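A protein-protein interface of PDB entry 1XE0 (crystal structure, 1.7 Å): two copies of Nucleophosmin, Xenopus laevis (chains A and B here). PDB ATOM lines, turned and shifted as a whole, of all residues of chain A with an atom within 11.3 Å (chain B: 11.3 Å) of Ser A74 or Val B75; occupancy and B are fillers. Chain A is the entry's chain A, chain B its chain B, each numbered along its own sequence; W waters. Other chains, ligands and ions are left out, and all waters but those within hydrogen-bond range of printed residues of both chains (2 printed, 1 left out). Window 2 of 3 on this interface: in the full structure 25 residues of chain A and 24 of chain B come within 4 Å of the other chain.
Leu A41 touches Leu B49, but with the chains exchanged Leu A49 does not touch Leu B41 (19.6 Å). Leu A41 touches Ser B70, but with the chains exchanged Ser A70 does not touch Leu B41 (17.7 Å). Val A75 touches its own counterpart, Val B75. Gln B76 touches its own counterpart, Gln A76. 18 positions are printed for both chains. Of the 14 pairs that touch across the chains among the printed residues, 2 have their exchanged pair printed and touching as well.
Of the 19 printed residues of chain B, 5 touch a printed residue of chain A. Among the printed residues, 14 pairs touch across the chains. Among the printed residues, no Asp or Glu carboxylate lies within 4 Å of a Lys or Arg side-chain nitrogen of the other chain.
O of Pro A77 is in hydrogen-bond range of N of Leu A41 (2.9 Å). The side-chain carboxylate (OD2) of Asp A47 is in hydrogen-bond range of the side-chain hydroxyl (OG) of Ser A74 (2.8 Å). The backbone NH (N) of Val B79 lies within hydrogen-bond range of the backbone carbonyl oxygen (O) of Val B39 (3.0 Å).
The backbone carbonyl oxygen (O) of Leu A41 sits at hydrogen-bond distance from the side-chain hydroxyl (OG) of Ser B70, at 2.7 Å. OG1 of Thr A78 sits at hydrogen-bond distance from O of Ser B70 (2.7 Å). OE1 of Gln B76 sits at hydrogen-bond distance from N of Thr A78, at 3.1 Å. OE1 of Gln B76 sits close to N of Pro A77 (3.4 Å).
Of the printed residues of chain B, Ser A40 touches Ser B70. Of the printed residues of chain B, Leu A41 touches Leu B49 (3.6 Å) and Ser B70 (2.7 Å). No residue of chain B comes within 4 Å of Lys A72. Ser A74 touches one residue of chain B. Of chain B, only Val B75 (3.4 Å) comes within 4 Å of Val A75. Printed residues of chain B within 4 Å of Gln A76: Gln B76 (3.9 Å). Printed residues of chain B within 4 Å of Thr A78: Ser B70 (2.7 Å), Gln B76 (3.1 Å) and Val B79 (3.9 Å). Of the printed residues of chain A, Val B75 touches Pro A73, Ser A74, Val A75 and Pro A77. Printed residues of chain A within 4 Å of Gln B76: Gln A76 (3.9 Å), Pro A77 (3.0 Å) and Thr A78 (3.1 Å). The nearest residue of chain B that does not touch Ser A74 is Ser B74 (5.6 Å).
Ser A40 touches Ser B70 (CB to OG, 3.4 Å). Leu B49 touches Leu A41 (CD2 to O, 3.6 Å). Leu B49 touches Ala A43. Pro A73 touches Val B75 (O to CG1, 3.96 Å). Val B75 touches Ser A74 (CG1 to O, 3.5 Å). Val B75 touches Val A75. Gln A76 touches Gln B76 (C to OE1, 3.9 Å). CG of Pro A77 touches O of Ser B70, at 3.6 Å. Val B75 touches Pro A77. Val B79 touches Thr A78 (CG2 to CB, 3.9 Å).
Water W2 lies within hydrogen-bond range of the side-chain hydroxyl of Ser B70 (2.6 Å), the side-chain hydroxyl of Ser A40 (2.8 Å) and the backbone carbonyl oxygen of Leu A41 (3.3 Å). Water W1 lies within hydrogen-bond range of O of Thr A78, NE2 of Gln B76 and NE2 of Gln A76.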
ATOM      1  N   SER A  40      13.015  20.344 -12.073  1.00  0.00           N
ATOM      2  CA  SER A  40      13.626  20.022 -13.372  1.00  0.00           C
ATOM      3  C   SER A  40      12.959  18.764 -13.948  1.00  0.00           C
ATOM      4  O   SER A  40      12.473  17.936 -13.244  1.00  0.00           O
ATOM      5  CB  SER A  40      15.125  19.806 -13.312  1.00  0.00           C
ATOM      6  OG  SER A  40      15.474  18.721 -12.380  1.00  0.00           O
ATOM      7  N   LEU A  41      12.992  18.707 -15.240  1.00  0.00           N
ATOM      8  CA  LEU A  41      12.478  17.595 -16.002  1.00  0.00           C
ATOM      9  C   LEU A  41      13.555  16.553 -16.256  1.00  0.00           C
ATOM     10  O   LEU A  41      14.644  16.837 -16.678  1.00  0.00           O
ATOM     11  CB  LEU A  41      11.906  18.098 -17.300  1.00  0.00           C
ATOM     12  CG  LEU A  41      10.657  18.997 -17.183  1.00  0.00           C
ATOM     13  CD1 LEU A  41      10.154  19.419 -18.481  1.00  0.00           C
ATOM     14  CD2 LEU A  41       9.557  18.387 -16.350  1.00  0.00           C
ATOM     15  N   GLY A  42      13.180  15.284 -16.042  1.00  0.00           N
ATOM     16  CA  GLY A  42      14.020  14.198 -16.344  1.00  0.00           C
ATOM     17  C   GLY A  42      14.142  13.939 -17.810  1.00  0.00           C
ATOM     18  O   GLY A  42      13.324  14.323 -18.580  1.00  0.00           O
ATOM     19  N   ALA A  43      15.218  13.216 -18.163  1.00  0.00           N
ATOM     20  CA  ALA A  43      15.640  12.988 -19.552  1.00  0.00           C
ATOM     21  C   ALA A  43      14.514  12.338 -20.359  1.00  0.00           C
ATOM     22  O   ALA A  43      14.343  12.576 -21.564  1.00  0.00           O
ATOM     23  CB  ALA A  43      16.886  12.033 -19.538  1.00  0.00           C
ATOM     24  N   SER A  44      13.720  11.543 -19.688  1.00  0.00           N
ATOM     25  CA  SER A  44      12.696  10.757 -20.387  1.00  0.00           C
ATOM     26  C   SER A  44      11.355  11.482 -20.589  1.00  0.00           C
ATOM     27  O   SER A  44      10.503  11.059 -21.342  1.00  0.00           O
ATOM     28  CB  SER A  44      12.546   9.384 -19.750  1.00  0.00           C
ATOM     29  OG  SER A  44      11.922   9.409 -18.426  1.00  0.00           O
ATOM     30  N   ALA A  45      11.164  12.606 -19.893  1.00  0.00           N
ATOM     31  CA  ALA A  45       9.917  13.347 -19.941  1.00  0.00           C
ATOM     32  C   ALA A  45       9.430  13.664 -21.295  1.00  0.00           C
ATOM     33  O   ALA A  45      10.175  14.186 -22.095  1.00  0.00           O
ATOM     34  CB  ALA A  45      10.072  14.650 -19.146  1.00  0.00           C
ATOM     35  N   LYS A  46       8.135  13.438 -21.519  1.00  0.00           N
ATOM     36  CA  LYS A  46       7.470  13.808 -22.746  1.00  0.00           C
ATOM     37  C   LYS A  46       7.418  15.307 -22.984  1.00  0.00           C
ATOM     38  O   LYS A  46       7.340  16.113 -21.995  1.00  0.00           O
ATOM     39  CB  LYS A  46       6.048  13.275 -22.724  1.00  0.00           C
ATOM     40  CG  LYS A  46       6.074  11.791 -23.048  1.00  0.00           C
ATOM     41  CD  LYS A  46       4.769  11.094 -22.746  1.00  0.00           C
ATOM     42  CE  LYS A  46       5.042   9.647 -22.346  1.00  0.00           C
ATOM     43  NZ  LYS A  46       5.239   8.652 -23.485  1.00  0.00           N
ATOM     44  N   ASP A  47       7.427  15.691 -24.260  1.00  0.00           N
ATOM     45  CA  ASP A  47       7.388  17.101 -24.624  1.00  0.00           C
ATOM     46  C   ASP A  47       6.012  17.775 -24.532  1.00  0.00           C
ATOM     47  O   ASP A  47       5.344  18.110 -25.505  1.00  0.00           O
ATOM     48  CB  ASP A  47       8.048  17.302 -25.981  1.00  0.00           C
ATOM     49  CG  ASP A  47       8.478  18.710 -26.193  1.00  0.00           C
ATOM     50  OD1 ASP A  47       8.596  19.465 -25.162  1.00  0.00           O
ATOM     51  OD2 ASP A  47       8.781  19.103 -27.325  1.00  0.00           O
ATOM     52  N   GLU A  48       5.606  18.074 -23.308  1.00  0.00           N
ATOM     53  CA  GLU A  48       4.323  18.644 -22.991  1.00  0.00           C
ATOM     54  C   GLU A  48       4.523  19.509 -21.758  1.00  0.00           C
ATOM     55  O   GLU A  48       5.546  19.385 -21.111  1.00  0.00           O
ATOM     56  CB  GLU A  48       3.326  17.566 -22.637  1.00  0.00           C
ATOM     57  CG  GLU A  48       3.813  16.550 -21.613  1.00  0.00           C
ATOM     58  CD  GLU A  48       2.965  15.308 -21.466  1.00  0.00           C
ATOM     59  OE1 GLU A  48       2.166  15.065 -22.348  1.00  0.00           O
ATOM     60  OE2 GLU A  48       3.165  14.574 -20.478  1.00  0.00           O
ATOM     61  N   LEU A  49       3.574  20.389 -21.444  1.00  0.00           N
ATOM     62  CA  LEU A  49       3.703  21.139 -20.206  1.00  0.00           C
ATOM     63  C   LEU A  49       3.538  20.190 -18.981  1.00  0.00           C
ATOM     64  O   LEU A  49       2.680  19.268 -18.903  1.00  0.00           O
ATOM     65  CB  LEU A  49       2.764  22.306 -20.200  1.00  0.00           C
ATOM     66  CG  LEU A  49       3.085  23.485 -19.272  1.00  0.00           C
ATOM     67  CD1 LEU A  49       4.323  24.322 -19.735  1.00  0.00           C
ATOM     68  CD2 LEU A  49       1.880  24.326 -19.272  1.00  0.00           C
ATOM     69  N   HIS A  50       4.404  20.398 -18.025  1.00  0.00           N
ATOM     70  CA  HIS A  50       4.351  19.730 -16.754  1.00  0.00           C
ATOM     71  C   HIS A  50       4.136  20.790 -15.709  1.00  0.00           C
ATOM     72  O   HIS A  50       4.816  21.761 -15.753  1.00  0.00           O
ATOM     73  CB  HIS A  50       5.648  18.955 -16.462  1.00  0.00           C
ATOM     74  CG  HIS A  50       5.956  17.898 -17.442  1.00  0.00           C
ATOM     75  ND1 HIS A  50       5.986  16.578 -17.101  1.00  0.00           N
ATOM     76  CD2 HIS A  50       6.372  17.982 -18.720  1.00  0.00           C
ATOM     77  CE1 HIS A  50       6.316  15.875 -18.165  1.00  0.00           C
ATOM     78  NE2 HIS A  50       6.554  16.698 -19.172  1.00  0.00           N
ATOM     79  N   SER A  70       5.567  25.693 -14.126  1.00  0.00           N
ATOM     80  CA  SER A  70       5.267  25.070 -15.417  1.00  0.00           C
ATOM     81  C   SER A  70       6.500  24.887 -16.306  1.00  0.00           C
ATOM     82  O   SER A  70       7.186  25.833 -16.595  1.00  0.00           O
ATOM     83  CB  SER A  70       4.295  26.021 -16.108  1.00  0.00           C
ATOM     84  OG  SER A  70       3.076  25.928 -15.399  1.00  0.00           O
ATOM     85  N   LEU A  71       6.840  23.642 -16.662  1.00  0.00           N
ATOM     86  CA  LEU A  71       8.040  23.370 -17.381  1.00  0.00           C
ATOM     87  C   LEU A  71       7.749  22.500 -18.619  1.00  0.00           C
ATOM     88  O   LEU A  71       6.777  21.796 -18.658  1.00  0.00           O
ATOM     89  CB  LEU A  71       8.943  22.523 -16.508  1.00  0.00           C
ATOM     90  CG  LEU A  71       9.229  23.026 -15.089  1.00  0.00           C
ATOM     91  CD1 LEU A  71      10.175  22.076 -14.397  1.00  0.00           C
ATOM     92  CD2 LEU A  71       9.826  24.342 -15.261  1.00  0.00           C
ATOM     93  N   LYS A  72       8.596  22.585 -19.599  1.00  0.00           N
ATOM     94  CA  LYS A  72       8.460  21.757 -20.883  1.00  0.00           C
ATOM     95  C   LYS A  72       9.827  21.506 -21.434  1.00  0.00           C
ATOM     96  O   LYS A  72      10.659  22.407 -21.442  1.00  0.00           O
ATOM     97  CB  LYS A  72       7.641  22.474 -21.888  1.00  0.00           C
ATOM     98  CG  LYS A  72       7.486  21.760 -23.238  1.00  0.00           C
ATOM     99  CD  LYS A  72       6.414  22.419 -24.173  1.00  0.00           C
ATOM    100  CE  LYS A  72       5.889  21.333 -25.201  1.00  0.00           C
ATOM    101  NZ  LYS A  72       5.219  21.795 -26.498  1.00  0.00           N
ATOM    102  N   PRO A  73      10.148  20.289 -21.823  1.00  0.00           N
ATOM    103  CA  PRO A  73      11.528  19.968 -22.167  1.00  0.00           C
ATOM    104  C   PRO A  73      12.089  20.769 -23.252  1.00  0.00           C
ATOM    105  O   PRO A  73      13.225  21.085 -23.167  1.00  0.00           O
ATOM    106  CB  PRO A  73      11.503  18.480 -22.523  1.00  0.00           C
ATOM    107  CG  PRO A  73      10.246  18.030 -22.199  1.00  0.00           C
ATOM    108  CD  PRO A  73       9.254  19.113 -21.885  1.00  0.00           C
ATOM    109  N   SER A  74      11.307  21.123 -24.234  1.00  0.00           N
ATOM    110  CA  SER A  74      11.873  21.749 -25.395  1.00  0.00           C
ATOM    111  C   SER A  74      11.795  23.281 -25.271  1.00  0.00           C
ATOM    112  O   SER A  74      12.232  24.021 -26.174  1.00  0.00           O
ATOM    113  CB  SER A  74      11.184  21.204 -26.630  1.00  0.00           C
ATOM    114  OG  SER A  74       9.850  21.638 -26.645  1.00  0.00           O
ATOM    115  N   VAL A  75      11.333  23.768 -24.109  1.00  0.00           N
ATOM    116  CA  VAL A  75      11.163  25.224 -23.856  1.00  0.00           C
ATOM    117  C   VAL A  75      11.932  25.724 -22.601  1.00  0.00           C
ATOM    118  O   VAL A  75      12.644  26.728 -22.648  1.00  0.00           O
ATOM    119  CB  VAL A  75       9.701  25.529 -23.690  1.00  0.00           C
ATOM    120  CG1 VAL A  75       9.457  26.958 -23.388  1.00  0.00           C
ATOM    121  CG2 VAL A  75       8.987  25.155 -25.055  1.00  0.00           C
ATOM    122  N   GLN A  76      11.739  24.990 -21.520  1.00  0.00           N
ATOM    123  CA  GLN A  76      12.171  25.471 -20.176  1.00  0.00           C
ATOM    124  C   GLN A  76      12.137  24.201 -19.276  1.00  0.00           C
ATOM    125  O   GLN A  76      11.191  23.935 -18.577  1.00  0.00           O
ATOM    126  CB  GLN A  76      11.195  26.529 -19.631  1.00  0.00           C
ATOM    127  CG  GLN A  76      11.719  27.202 -18.313  1.00  0.00           C
ATOM    128  CD  GLN A  76      10.857  28.285 -17.768  1.00  0.00           C
ATOM    129  OE1 GLN A  76       9.745  28.490 -18.176  1.00  0.00           O
ATOM    130  NE2 GLN A  76      11.421  29.052 -16.833  1.00  0.00           N
ATOM    131  N   PRO A  77      13.169  23.397 -19.352  1.00  0.00           N
ATOM    132  CA  PRO A  77      13.241  22.160 -18.587  1.00  0.00           C
ATOM    133  C   PRO A  77      13.567  22.358 -17.085  1.00  0.00           C
ATOM    134  O   PRO A  77      13.454  21.382 -16.384  1.00  0.00           O
ATOM    135  CB  PRO A  77      14.356  21.377 -19.285  1.00  0.00           C
ATOM    136  CG  PRO A  77      15.216  22.317 -19.959  1.00  0.00           C
ATOM    137  CD  PRO A  77      14.265  23.491 -20.310  1.00  0.00           C
ATOM    138  N   THR A  78      14.043  23.543 -16.662  1.00  0.00           N
ATOM    139  CA  THR A  78      14.422  23.709 -15.231  1.00  0.00           C
ATOM    140  C   THR A  78      13.912  25.058 -14.808  1.00  0.00           C
ATOM    141  O   THR A  78      14.066  26.006 -15.569  1.00  0.00           O
ATOM    142  CB  THR A  78      15.908  23.697 -15.018  1.00  0.00           C
ATOM    143  OG1 THR A  78      16.445  22.427 -15.437  1.00  0.00           O
ATOM    144  CG2 THR A  78      16.228  23.747 -13.564  1.00  0.00           C
ATOM    145  N   VAL A  79      13.373  25.192 -13.615  1.00  0.00           N
ATOM    146  CA  VAL A  79      13.137  26.481 -13.010  1.00  0.00           C
ATOM    147  C   VAL A  79      13.784  26.526 -11.639  1.00  0.00           C
ATOM    148  O   VAL A  79      13.619  25.553 -10.850  1.00  0.00           O
ATOM    149  CB  VAL A  79      11.575  26.674 -12.828  1.00  0.00           C
ATOM    150  CG1 VAL A  79      11.198  27.727 -11.836  1.00  0.00           C
ATOM    151  CG2 VAL A  79      10.975  26.923 -14.151  1.00  0.00           C
ATOM    152  N   VAL B  39      24.982  26.446 -13.198  1.00  0.00           N
ATOM    153  CA  VAL B  39      25.371  25.290 -13.940  1.00  0.00           C
ATOM    154  C   VAL B  39      25.192  25.656 -15.374  1.00  0.00           C
ATOM    155  O   VAL B  39      24.205  26.266 -15.713  1.00  0.00           O
ATOM    156  CB  VAL B  39      24.456  24.140 -13.611  1.00  0.00           C
ATOM    157  CG1 VAL B  39      24.957  22.840 -14.229  1.00  0.00           C
ATOM    158  CG2 VAL B  39      24.279  24.014 -12.072  1.00  0.00           C
ATOM    159  N   SER B  40      26.137  25.287 -16.213  1.00  0.00           N
ATOM    160  CA  SER B  40      26.102  25.818 -17.603  1.00  0.00           C
ATOM    161  C   SER B  40      26.755  24.789 -18.523  1.00  0.00           C
ATOM    162  O   SER B  40      27.595  24.054 -18.110  1.00  0.00           O
ATOM    163  CB  SER B  40      26.896  27.098 -17.754  1.00  0.00           C
ATOM    164  OG  SER B  40      28.267  27.006 -17.429  1.00  0.00           O
ATOM    165  N   LEU B  41      26.375  24.824 -19.765  1.00  0.00           N
ATOM    166  CA  LEU B  41      26.885  23.836 -20.702  1.00  0.00           C
ATOM    167  C   LEU B  41      28.054  24.430 -21.456  1.00  0.00           C
ATOM    168  O   LEU B  41      27.959  25.542 -21.912  1.00  0.00           O
ATOM    169  CB  LEU B  41      25.806  23.418 -21.649  1.00  0.00           C
ATOM    170  CG  LEU B  41      24.664  22.638 -21.027  1.00  0.00           C
ATOM    171  CD1 LEU B  41      23.661  22.243 -22.003  1.00  0.00           C
ATOM    172  CD2 LEU B  41      25.166  21.396 -20.310  1.00  0.00           C
ATOM    173  N   ALA B  45      29.348  20.626 -25.704  1.00  0.00           N
ATOM    174  CA  ALA B  45      28.246  19.801 -25.295  1.00  0.00           C
ATOM    175  C   ALA B  45      27.392  19.495 -26.504  1.00  0.00           C
ATOM    176  O   ALA B  45      27.100  20.369 -27.307  1.00  0.00           O
ATOM    177  CB  ALA B  45      27.357  20.549 -24.202  1.00  0.00           C
ATOM    178  N   LYS B  46      26.963  18.254 -26.605  1.00  0.00           N
ATOM    179  CA  LYS B  46      26.089  17.833 -27.652  1.00  0.00           C
ATOM    180  C   LYS B  46      24.708  18.351 -27.339  1.00  0.00           C
ATOM    181  O   LYS B  46      24.386  18.758 -26.197  1.00  0.00           O
ATOM    182  CB  LYS B  46      26.101  16.305 -27.801  1.00  0.00           C
ATOM    183  CG  LYS B  46      27.418  15.766 -28.398  1.00  0.00           C
ATOM    184  CD  LYS B  46      27.311  14.270 -28.622  1.00  0.00           C
ATOM    185  CE  LYS B  46      28.609  13.519 -28.168  1.00  0.00           C
ATOM    186  NZ  LYS B  46      28.397  12.021 -28.328  1.00  0.00           N
ATOM    187  N   ASP B  47      23.883  18.417 -28.361  1.00  0.00           N
ATOM    188  CA  ASP B  47      22.548  18.963 -28.190  1.00  0.00           C
ATOM    189  C   ASP B  47      21.540  17.902 -27.767  1.00  0.00           C
ATOM    190  O   ASP B  47      20.691  17.437 -28.523  1.00  0.00           O
ATOM    191  CB  ASP B  47      22.129  19.778 -29.422  1.00  0.00           C
ATOM    192  CG  ASP B  47      20.944  20.682 -29.158  1.00  0.00           C
ATOM    193  OD1 ASP B  47      20.181  20.937 -30.124  1.00  0.00           O
ATOM    194  OD2 ASP B  47      20.707  21.270 -28.060  1.00  0.00           O
ATOM    195  N   GLU B  48      21.577  17.613 -26.462  1.00  0.00           N
ATOM    196  CA  GLU B  48      20.745  16.656 -25.780  1.00  0.00           C
ATOM    197  C   GLU B  48      20.564  17.218 -24.363  1.00  0.00           C
ATOM    198  O   GLU B  48      21.334  18.089 -23.981  1.00  0.00           O
ATOM    199  CB  GLU B  48      21.475  15.300 -25.676  1.00  0.00           C
ATOM    200  CG  GLU B  48      22.925  15.379 -25.270  1.00  0.00           C
ATOM    201  CD  GLU B  48      23.675  14.075 -25.264  1.00  0.00           C
ATOM    202  OE1 GLU B  48      24.811  14.094 -24.729  1.00  0.00           O
ATOM    203  OE2 GLU B  48      23.252  13.088 -25.900  1.00  0.00           O
ATOM    204  N   LEU B  49      19.573  16.730 -23.631  1.00  0.00           N
ATOM    205  CA  LEU B  49      19.503  16.976 -22.175  1.00  0.00           C
ATOM    206  C   LEU B  49      20.737  16.493 -21.399  1.00  0.00           C
ATOM    207  O   LEU B  49      21.323  15.402 -21.639  1.00  0.00           O
ATOM    208  CB  LEU B  49      18.165  16.528 -21.581  1.00  0.00           C
ATOM    209  CG  LEU B  49      17.811  17.311 -20.340  1.00  0.00           C
ATOM    210  CD1 LEU B  49      17.116  18.746 -20.686  1.00  0.00           C
ATOM    211  CD2 LEU B  49      16.927  16.495 -19.452  1.00  0.00           C
ATOM    212  N   HIS B  50      21.177  17.388 -20.502  1.00  0.00           N
ATOM    213  CA  HIS B  50      22.209  17.160 -19.543  1.00  0.00           C
ATOM    214  C   HIS B  50      21.570  17.298 -18.176  1.00  0.00           C
ATOM    215  O   HIS B  50      20.876  18.269 -17.913  1.00  0.00           O
ATOM    216  CB  HIS B  50      23.332  18.145 -19.700  1.00  0.00           C
ATOM    217  CG  HIS B  50      24.021  17.994 -20.993  1.00  0.00           C
ATOM    218  ND1 HIS B  50      25.303  17.530 -21.129  1.00  0.00           N
ATOM    219  CD2 HIS B  50      23.592  18.313 -22.234  1.00  0.00           C
ATOM    220  CE1 HIS B  50      25.645  17.558 -22.407  1.00  0.00           C
ATOM    221  NE2 HIS B  50      24.622  18.028 -23.101  1.00  0.00           N
ATOM    222  N   SER B  70      18.423  20.447 -15.255  1.00  0.00           N
ATOM    223  CA  SER B  70      18.390  19.831 -16.559  1.00  0.00           C
ATOM    224  C   SER B  70      18.644  20.901 -17.604  1.00  0.00           C
ATOM    225  O   SER B  70      17.906  21.846 -17.635  1.00  0.00           O
ATOM    226  CB  SER B  70      16.962  19.245 -16.758  1.00  0.00           C
ATOM    227  OG  SER B  70      16.805  18.201 -15.790  1.00  0.00           O
ATOM    228  N   LEU B  71      19.665  20.727 -18.435  1.00  0.00           N
ATOM    229  CA  LEU B  71      20.042  21.795 -19.362  1.00  0.00           C
ATOM    230  C   LEU B  71      20.154  21.224 -20.777  1.00  0.00           C
ATOM    231  O   LEU B  71      20.342  20.061 -20.949  1.00  0.00           O
ATOM    232  CB  LEU B  71      21.374  22.352 -18.943  1.00  0.00           C
ATOM    233  CG  LEU B  71      21.505  22.944 -17.583  1.00  0.00           C
ATOM    234  CD1 LEU B  71      22.888  23.407 -17.445  1.00  0.00           C
ATOM    235  CD2 LEU B  71      20.617  24.136 -17.558  1.00  0.00           C
ATOM    236  N   LYS B  72      20.046  22.070 -21.787  1.00  0.00           N
ATOM    237  CA  LYS B  72      20.190  21.601 -23.162  1.00  0.00           C
ATOM    238  C   LYS B  72      20.624  22.800 -23.975  1.00  0.00           C
ATOM    239  O   LYS B  72      20.042  23.862 -23.789  1.00  0.00           O
ATOM    240  CB  LYS B  72      18.799  21.210 -23.656  1.00  0.00           C
ATOM    241  CG  LYS B  72      18.833  20.731 -25.152  1.00  0.00           C
ATOM    242  CD  LYS B  72      17.662  19.703 -25.379  1.00  0.00           C
ATOM    243  CE  LYS B  72      18.072  18.767 -26.520  1.00  0.00           C
ATOM    244  NZ  LYS B  72      18.325  19.452 -27.830  1.00  0.00           N
ATOM    245  N   PRO B  73      21.647  22.687 -24.800  1.00  0.00           N
ATOM    246  CA  PRO B  73      22.232  23.865 -25.415  1.00  0.00           C
ATOM    247  C   PRO B  73      21.306  24.699 -26.307  1.00  0.00           C
ATOM    248  O   PRO B  73      21.518  25.921 -26.295  1.00  0.00           O
ATOM    249  CB  PRO B  73      23.376  23.265 -26.272  1.00  0.00           C
ATOM    250  CG  PRO B  73      23.646  21.965 -25.743  1.00  0.00           C
ATOM    251  CD  PRO B  73      22.410  21.489 -25.182  1.00  0.00           C
ATOM    252  N   SER B  74      20.359  24.136 -27.001  1.00  0.00           N
ATOM    253  CA  SER B  74      19.478  24.923 -27.830  1.00  0.00           C
ATOM    254  C   SER B  74      18.179  25.341 -27.143  1.00  0.00           C
ATOM    255  O   SER B  74      17.279  25.926 -27.758  1.00  0.00           O
ATOM    256  CB  SER B  74      19.198  24.069 -29.087  1.00  0.00           C
ATOM    257  OG  SER B  74      18.511  22.903 -28.680  1.00  0.00           O
ATOM    258  N   VAL B  75      18.003  25.019 -25.850  1.00  0.00           N
ATOM    259  CA  VAL B  75      16.832  25.441 -25.130  1.00  0.00           C
ATOM    260  C   VAL B  75      17.196  26.247 -23.854  1.00  0.00           C
ATOM    261  O   VAL B  75      16.537  27.224 -23.538  1.00  0.00           O
ATOM    262  CB  VAL B  75      16.042  24.210 -24.684  1.00  0.00           C
ATOM    263  CG1 VAL B  75      14.864  24.587 -24.015  1.00  0.00           C
ATOM    264  CG2 VAL B  75      15.695  23.379 -25.993  1.00  0.00           C
ATOM    265  N   GLN B  76      18.120  25.750 -23.094  1.00  0.00           N
ATOM    266  CA  GLN B  76      18.459  26.382 -21.784  1.00  0.00           C
ATOM    267  C   GLN B  76      19.888  25.970 -21.360  1.00  0.00           C
ATOM    268  O   GLN B  76      20.047  24.988 -20.642  1.00  0.00           O
ATOM    269  CB  GLN B  76      17.388  25.961 -20.751  1.00  0.00           C
ATOM    270  CG  GLN B  76      17.561  26.611 -19.338  1.00  0.00           C
ATOM    271  CD  GLN B  76      16.495  26.309 -18.339  1.00  0.00           C
ATOM    272  OE1 GLN B  76      15.768  25.341 -18.447  1.00  0.00           O
ATOM    273  NE2 GLN B  76      16.536  27.043 -17.210  1.00  0.00           N
ATOM    274  N   PRO B  77      20.911  26.666 -21.877  1.00  0.00           N
ATOM    275  CA  PRO B  77      22.328  26.358 -21.655  1.00  0.00           C
ATOM    276  C   PRO B  77      22.838  26.645 -20.275  1.00  0.00           C
ATOM    277  O   PRO B  77      23.841  26.126 -19.893  1.00  0.00           O
ATOM    278  CB  PRO B  77      23.061  27.151 -22.739  1.00  0.00           C
ATOM    279  CG  PRO B  77      22.132  28.282 -23.056  1.00  0.00           C
ATOM    280  CD  PRO B  77      20.759  27.761 -22.873  1.00  0.00           C
ATOM    281  N   THR B  78      22.182  27.544 -19.576  1.00  0.00           N
ATOM    282  CA  THR B  78      22.580  27.920 -18.179  1.00  0.00           C
ATOM    283  C   THR B  78      21.367  28.001 -17.225  1.00  0.00           C
ATOM    284  O   THR B  78      20.309  28.467 -17.572  1.00  0.00           O
ATOM    285  CB  THR B  78      23.205  29.303 -18.209  1.00  0.00           C
ATOM    286  OG1 THR B  78      24.341  29.251 -19.025  1.00  0.00           O
ATOM    287  CG2 THR B  78      23.720  29.735 -16.843  1.00  0.00           C
ATOM    288  N   VAL B  79      21.535  27.554 -15.965  1.00  0.00           N
ATOM    289  CA  VAL B  79      20.594  27.727 -14.950  1.00  0.00           C
ATOM    290  C   VAL B  79      21.305  28.388 -13.781  1.00  0.00           C
ATOM    291  O   VAL B  79      22.377  27.918 -13.356  1.00  0.00           O
ATOM    292  CB  VAL B  79      20.044  26.312 -14.497  1.00  0.00           C
ATOM    293  CG1 VAL B  79      19.451  26.326 -13.171  1.00  0.00           C
ATOM    294  CG2 VAL B  79      19.071  25.893 -15.525  1.00  0.00           C
HETATM  295  O   HOH W   1      14.437  28.869 -15.937  1.00  0.00           O
HETATM  296  O   HOH W   2      16.447  16.519 -13.891  1.00  0.00           O
